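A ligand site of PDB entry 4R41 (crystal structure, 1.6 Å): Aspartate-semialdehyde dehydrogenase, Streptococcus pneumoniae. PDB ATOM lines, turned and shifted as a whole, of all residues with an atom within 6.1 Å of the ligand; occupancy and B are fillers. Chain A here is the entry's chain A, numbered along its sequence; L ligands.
The guanidinium group (NH2) of Arg 99 lies within salt-bridge range of an oxygen (O7) of the ligand, 2.8 Å away.
O6 of the ligand is in salt-bridge range of NZ of Lys 223 (2.7 Å).
The backbone NH of Gly 73 lies within hydrogen-bond range of an oxygen (O5) of the ligand (3.0 Å).
An oxygen (O1) of the ligand is in hydrogen-bond range of the side-chain hydroxyl (OG) of Ser 96 (2.7 Å).
OG of Ser 74 is in hydrogen-bond range of O1 of the ligand (2.6 Å).
The side-chain amide nitrogen (ND2) of Asn 127 lies within hydrogen-bond range of an oxygen (O7) of the ligand (3.0 Å).
An oxygen (O1) of the ligand is in hydrogen-bond range of the backbone NH (N) of Ser 96.
The backbone NH of Ser 74 is in hydrogen-bond range of an oxygen (O2) of the ligand (2.8 Å).
N of Ala 72 sits at hydrogen-bond distance from O5 of the ligand (3.4 Å).
N of Tyr 97 lies close to OG1 of Thr 95, 3.3 Å away.
NZ of Lys 223 lies within salt-bridge range of OD2 of Asp 210, 2.7 Å away.
The backbone NH (N) of Asn 127 sits at hydrogen-bond distance from the side-chain carboxylate (OE1) of Glu 227, at 2.8 Å.
The backbone NH of Asn 94 lies within hydrogen-bond range of the backbone carbonyl oxygen of Phe 70 (3.0 Å).
OG of Ser 74 is in hydrogen-bond range of N of Tyr 97.
The guanidinium group (NH1) of Arg 99 lies within salt-bridge range of the side-chain carboxylate (OE2) of Glu 227 (2.8 Å).
The backbone carbonyl oxygen (O) of Ala 330 sits close to the side-chain amide oxygen (OD1) of Asn 94, 3.2 Å away.
The guanidinium group of Arg 99 sits at hydrogen-bond distance from the backbone carbonyl oxygen of Asn 94.
CG2 of Val 14 touches O4 of the ligand (3.5 Å).
Ser 71 touches the ligand.
Asn 94 touches the ligand (O to C4, 3.4 Å).
CG2 of Thr 95 touches O5 of the ligand, at 3.7 Å.
Hydrophobic or aromatic side chains that line the ligand: Val 14.
Of the 21 residues printed, 11 come within 4 Å of the ligand.
The nearest printed residue that does not touch the ligand is Asp 210 (4.2 Å).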
ATOM      1  N   VAL A  14      26.606  -1.928   9.604  1.00  0.00           N
ATOM      2  CA  VAL A  14      27.009  -3.296   9.204  1.00  0.00           C
ATOM      3  C   VAL A  14      28.289  -3.690   9.941  1.00  0.00           C
ATOM      4  O   VAL A  14      28.382  -4.790  10.491  1.00  0.00           O
ATOM      5  CB  VAL A  14      27.195  -3.455   7.664  1.00  0.00           C
ATOM      6  CG1 VAL A  14      27.797  -4.824   7.320  1.00  0.00           C
ATOM      7  CG2 VAL A  14      25.874  -3.264   6.913  1.00  0.00           C
ATOM      8  N   PHE A  70      34.657  -5.989   3.730  1.00  0.00           N
ATOM      9  CA  PHE A  70      34.329  -4.588   3.386  1.00  0.00           C
ATOM     10  C   PHE A  70      32.849  -4.299   3.584  1.00  0.00           C
ATOM     11  O   PHE A  70      31.977  -4.957   3.001  1.00  0.00           O
ATOM     12  CB  PHE A  70      34.690  -4.278   1.935  1.00  0.00           C
ATOM     13  CG  PHE A  70      36.147  -3.937   1.702  1.00  0.00           C
ATOM     14  CD1 PHE A  70      37.145  -4.916   1.820  1.00  0.00           C
ATOM     15  CD2 PHE A  70      36.520  -2.654   1.277  1.00  0.00           C
ATOM     16  CE1 PHE A  70      38.474  -4.583   1.541  1.00  0.00           C
ATOM     17  CE2 PHE A  70      37.843  -2.319   1.017  1.00  0.00           C
ATOM     18  CZ  PHE A  70      38.817  -3.302   1.139  1.00  0.00           C
ATOM     19  N   SER A  71      32.568  -3.300   4.410  1.00  0.00           N
ATOM     20  CA  SER A  71      31.201  -2.800   4.556  1.00  0.00           C
ATOM     21  C   SER A  71      31.217  -1.289   4.771  1.00  0.00           C
ATOM     22  O   SER A  71      30.665  -0.767   5.753  1.00  0.00           O
ATOM     23  CB  SER A  71      30.470  -3.532   5.671  1.00  0.00           C
ATOM     24  OG  SER A  71      31.102  -3.276   6.913  1.00  0.00           O
ATOM     25  N   ALA A  72      31.851  -0.598   3.841  1.00  0.00           N
ATOM     26  CA  ALA A  72      32.057   0.838   3.939  1.00  0.00           C
ATOM     27  C   ALA A  72      31.532   1.612   2.722  1.00  0.00           C
ATOM     28  O   ALA A  72      31.980   2.732   2.460  1.00  0.00           O
ATOM     29  CB  ALA A  72      33.535   1.141   4.196  1.00  0.00           C
ATOM     30  N   GLY A  73      30.612   0.994   1.966  1.00  0.00           N
ATOM     31  CA  GLY A  73      30.008   1.660   0.800  1.00  0.00           C
ATOM     32  C   GLY A  73      30.760   1.316  -0.467  1.00  0.00           C
ATOM     33  O   GLY A  73      31.984   1.144  -0.456  1.00  0.00           O
ATOM     34  N   SER A  74      30.008   1.219  -1.571  1.00  0.00           N
ATOM     35  CA  SER A  74      30.586   0.924  -2.881  1.00  0.00           C
ATOM     36  C   SER A  74      31.844   1.718  -3.246  1.00  0.00           C
ATOM     37  O   SER A  74      32.792   1.157  -3.778  1.00  0.00           O
ATOM     38  CB  SER A  74      29.538   1.108  -3.981  1.00  0.00           C
ATOM     39  OG  SER A  74      28.737  -0.044  -4.089  1.00  0.00           O
ATOM     40  N   SER A  75      31.846   3.020  -2.963  1.00  0.00           N
ATOM     41  CA  SER A  75      32.994   3.818  -3.381  1.00  0.00           C
ATOM     42  C   SER A  75      34.269   3.374  -2.671  1.00  0.00           C
ATOM     43  O   SER A  75      35.320   3.272  -3.301  1.00  0.00           O
ATOM     44  CB  SER A  75      32.730   5.307  -3.182  1.00  0.00           C
ATOM     45  OG  SER A  75      33.933   6.035  -3.337  1.00  0.00           O
ATOM     46  N   ASN A  94      30.660  -6.616   0.936  1.00  0.00           N
ATOM     47  CA  ASN A  94      29.191  -6.459   1.097  1.00  0.00           C
ATOM     48  C   ASN A  94      28.517  -5.525   0.094  1.00  0.00           C
ATOM     49  O   ASN A  94      27.270  -5.535  -0.031  1.00  0.00           O
ATOM     50  CB  ASN A  94      28.842  -5.968   2.485  1.00  0.00           C
ATOM     51  CG  ASN A  94      28.811  -7.067   3.501  1.00  0.00           C
ATOM     52  OD1 ASN A  94      27.871  -7.885   3.562  1.00  0.00           O
ATOM     53  ND2 ASN A  94      29.831  -7.109   4.298  1.00  0.00           N
ATOM     54  N   THR A  95      29.312  -4.705  -0.604  1.00  0.00           N
ATOM     55  CA  THR A  95      28.734  -3.620  -1.396  1.00  0.00           C
ATOM     56  C   THR A  95      28.257  -4.097  -2.771  1.00  0.00           C
ATOM     57  O   THR A  95      28.525  -5.219  -3.171  1.00  0.00           O
ATOM     58  CB  THR A  95      29.695  -2.412  -1.582  1.00  0.00           C
ATOM     59  OG1 THR A  95      30.633  -2.723  -2.611  1.00  0.00           O
ATOM     60  CG2 THR A  95      30.433  -2.045  -0.279  1.00  0.00           C
ATOM     61  N   SER A  96      27.563  -3.222  -3.502  1.00  0.00           N
ATOM     62  CA  SER A  96      27.083  -3.610  -4.834  1.00  0.00           C
ATOM     63  C   SER A  96      28.183  -3.595  -5.911  1.00  0.00           C
ATOM     64  O   SER A  96      27.974  -4.119  -7.006  1.00  0.00           O
ATOM     65  CB  SER A  96      25.936  -2.679  -5.241  1.00  0.00           C
ATOM     66  OG  SER A  96      26.433  -1.368  -5.423  1.00  0.00           O
ATOM     67  N   TYR A  97      29.349  -3.020  -5.601  1.00  0.00           N
ATOM     68  CA  TYR A  97      30.291  -2.611  -6.646  1.00  0.00           C
ATOM     69  C   TYR A  97      30.732  -3.731  -7.582  1.00  0.00           C
ATOM     70  O   TYR A  97      30.706  -3.579  -8.816  1.00  0.00           O
ATOM     71  CB  TYR A  97      31.516  -1.866  -6.097  1.00  0.00           C
ATOM     72  CG  TYR A  97      32.276  -1.166  -7.221  1.00  0.00           C
ATOM     73  CD1 TYR A  97      31.800   0.034  -7.765  1.00  0.00           C
ATOM     74  CD2 TYR A  97      33.423  -1.741  -7.778  1.00  0.00           C
ATOM     75  CE1 TYR A  97      32.484   0.662  -8.810  1.00  0.00           C
ATOM     76  CE2 TYR A  97      34.105  -1.127  -8.823  1.00  0.00           C
ATOM     77  CZ  TYR A  97      33.634   0.075  -9.334  1.00  0.00           C
ATOM     78  OH  TYR A  97      34.320   0.683 -10.367  1.00  0.00           O
ATOM     79  N   ARG A  99      29.467  -6.918  -7.720  1.00  0.00           N
ATOM     80  CA  ARG A  99      28.561  -8.065  -7.722  1.00  0.00           C
ATOM     81  C   ARG A  99      28.351  -8.691  -9.101  1.00  0.00           C
ATOM     82  O   ARG A  99      28.166  -9.901  -9.183  1.00  0.00           O
ATOM     83  CB  ARG A  99      27.192  -7.669  -7.159  1.00  0.00           C
ATOM     84  CG  ARG A  99      27.223  -7.378  -5.674  1.00  0.00           C
ATOM     85  CD  ARG A  99      25.796  -7.339  -5.125  1.00  0.00           C
ATOM     86  NE  ARG A  99      25.817  -6.902  -3.730  1.00  0.00           N
ATOM     87  CZ  ARG A  99      25.069  -5.940  -3.221  1.00  0.00           C
ATOM     88  NH1 ARG A  99      24.133  -5.341  -3.964  1.00  0.00           N
ATOM     89  NH2 ARG A  99      25.228  -5.598  -1.924  1.00  0.00           N
ATOM     90  N   PRO A 126      25.615 -10.676  -1.816  1.00  0.00           N
ATOM     91  CA  PRO A 126      24.500 -10.016  -2.511  1.00  0.00           C
ATOM     92  C   PRO A 126      23.862  -8.967  -1.614  1.00  0.00           C
ATOM     93  O   PRO A 126      24.194  -8.840  -0.435  1.00  0.00           O
ATOM     94  CB  PRO A 126      23.510 -11.148  -2.800  1.00  0.00           C
ATOM     95  CG  PRO A 126      24.272 -12.426  -2.574  1.00  0.00           C
ATOM     96  CD  PRO A 126      25.339 -12.103  -1.549  1.00  0.00           C
ATOM     97  N   ASN A 127      22.948  -8.212  -2.199  1.00  0.00           N
ATOM     98  CA  ASN A 127      22.151  -7.244  -1.475  1.00  0.00           C
ATOM     99  C   ASN A 127      21.304  -7.965  -0.415  1.00  0.00           C
ATOM    100  O   ASN A 127      20.879  -9.101  -0.635  1.00  0.00           O
ATOM    101  CB  ASN A 127      21.240  -6.544  -2.491  1.00  0.00           C
ATOM    102  CG  ASN A 127      20.222  -5.673  -1.832  1.00  0.00           C
ATOM    103  OD1 ASN A 127      19.093  -6.107  -1.611  1.00  0.00           O
ATOM    104  ND2 ASN A 127      20.619  -4.460  -1.459  1.00  0.00           N
ATOM    105  N   CYS A 128      21.057  -7.294   0.724  1.00  0.00           N
ATOM    106  CA  CYS A 128      20.354  -7.921   1.858  1.00  0.00           C
ATOM    107  C   CYS A 128      18.982  -8.516   1.482  1.00  0.00           C
ATOM    108  O   CYS A 128      18.622  -9.652   1.896  1.00  0.00           O
ATOM    109  CB  CYS A 128      20.183  -6.881   3.004  1.00  0.00           C
ATOM    110  SG  CYS A 128      19.645  -5.246   2.432  1.00  0.00           S
ATOM    111  N   GLY A 159      19.647  -0.693   6.820  1.00  0.00           N
ATOM    112  CA  GLY A 159      20.296  -0.924   5.544  1.00  0.00           C
ATOM    113  C   GLY A 159      20.871   0.336   4.929  1.00  0.00           C
ATOM    114  O   GLY A 159      21.768   0.249   4.097  1.00  0.00           O
ATOM    115  N   ASP A 210      17.628   3.137  -2.971  1.00  0.00           N
ATOM    116  CA  ASP A 210      18.710   3.520  -3.900  1.00  0.00           C
ATOM    117  C   ASP A 210      18.166   4.561  -4.876  1.00  0.00           C
ATOM    118  O   ASP A 210      17.079   5.086  -4.663  1.00  0.00           O
ATOM    119  CB  ASP A 210      19.301   2.273  -4.614  1.00  0.00           C
ATOM    120  CG  ASP A 210      20.793   2.406  -4.890  1.00  0.00           C
ATOM    121  OD1 ASP A 210      21.223   3.405  -5.542  1.00  0.00           O
ATOM    122  OD2 ASP A 210      21.546   1.491  -4.473  1.00  0.00           O
ATOM    123  N   GLU A 220      17.872  -0.718  -6.374  1.00  0.00           N
ATOM    124  CA  GLU A 220      17.570  -1.802  -5.437  1.00  0.00           C
ATOM    125  C   GLU A 220      16.750  -2.886  -6.110  1.00  0.00           C
ATOM    126  O   GLU A 220      17.031  -4.084  -5.956  1.00  0.00           O
ATOM    127  CB  GLU A 220      16.842  -1.291  -4.190  1.00  0.00           C
ATOM    128  CG  GLU A 220      16.759  -2.336  -3.079  1.00  0.00           C
ATOM    129  CD  GLU A 220      18.019  -2.354  -2.206  1.00  0.00           C
ATOM    130  OE1 GLU A 220      19.065  -1.823  -2.658  1.00  0.00           O
ATOM    131  OE2 GLU A 220      17.958  -2.877  -1.045  1.00  0.00           O
ATOM    132  N   LYS A 223      18.980  -4.693  -8.610  1.00  0.00           N
ATOM    133  CA  LYS A 223      19.851  -5.618  -7.844  1.00  0.00           C
ATOM    134  C   LYS A 223      19.169  -6.958  -7.597  1.00  0.00           C
ATOM    135  O   LYS A 223      19.738  -8.018  -7.865  1.00  0.00           O
ATOM    136  CB  LYS A 223      20.309  -5.012  -6.508  1.00  0.00           C
ATOM    137  CG  LYS A 223      21.270  -3.827  -6.598  1.00  0.00           C
ATOM    138  CD  LYS A 223      21.462  -3.248  -5.200  1.00  0.00           C
ATOM    139  CE  LYS A 223      21.905  -1.800  -5.223  1.00  0.00           C
ATOM    140  NZ  LYS A 223      21.537  -1.182  -3.925  1.00  0.00           N
ATOM    141  N   GLU A 227      21.005 -10.018  -9.441  1.00  0.00           N
ATOM    142  CA  GLU A 227      21.694 -10.894  -8.492  1.00  0.00           C
ATOM    143  C   GLU A 227      21.016 -12.274  -8.427  1.00  0.00           C
ATOM    144  O   GLU A 227      21.693 -13.302  -8.396  1.00  0.00           O
ATOM    145  CB  GLU A 227      21.752 -10.227  -7.109  1.00  0.00           C
ATOM    146  CG  GLU A 227      22.577  -8.936  -7.154  1.00  0.00           C
ATOM    147  CD  GLU A 227      22.478  -8.118  -5.861  1.00  0.00           C
ATOM    148  OE1 GLU A 227      22.024  -8.656  -4.832  1.00  0.00           O
ATOM    149  OE2 GLU A 227      22.901  -6.946  -5.895  1.00  0.00           O
ATOM    150  N   ALA A 330      23.698  -9.237   5.624  1.00  0.00           N
ATOM    151  CA  ALA A 330      24.992  -8.557   5.468  1.00  0.00           C
ATOM    152  C   ALA A 330      26.144  -9.261   6.220  1.00  0.00           C
ATOM    153  O   ALA A 330      26.838 -10.092   5.642  1.00  0.00           O
ATOM    154  CB  ALA A 330      24.892  -7.072   5.840  1.00  0.00           C
HETATM  155  O1  LIG L   1      26.632  -0.724  -2.797  1.00  0.00           O
HETATM  156  P1  LIG L   1      26.185   0.042  -1.578  1.00  0.00           P
HETATM  157  O2  LIG L   1      27.268   1.015  -1.111  1.00  0.00           O
HETATM  158  O3  LIG L   1      24.840   0.753  -1.675  1.00  0.00           O
HETATM  159  C1  LIG L   1      25.947  -1.168  -0.328  1.00  0.00           C
HETATM  160  C2  LIG L   1      26.862  -1.145   0.725  1.00  0.00           C
HETATM  161  C3  LIG L   1      26.740  -2.075   1.761  1.00  0.00           C
HETATM  162  N1  LIG L   1      27.655  -2.067   2.805  1.00  0.00           N
HETATM  163  O4  LIG L   1      27.531  -3.005   3.821  1.00  0.00           O
HETATM  164  O5  LIG L   1      28.673  -1.120   2.806  1.00  0.00           O
HETATM  165  C4  LIG L   1      25.738  -3.059   1.768  1.00  0.00           C
HETATM  166  C5  LIG L   1      24.829  -3.089   0.718  1.00  0.00           C
HETATM  167  C6  LIG L   1      24.931  -2.150  -0.325  1.00  0.00           C
HETATM  168  C7  LIG L   1      23.886  -2.299  -1.382  1.00  0.00           C
HETATM  169  O6  LIG L   1      23.457  -1.301  -1.987  1.00  0.00           O
HETATM  170  O7  LIG L   1      23.437  -3.449  -1.629  1.00  0.00           O
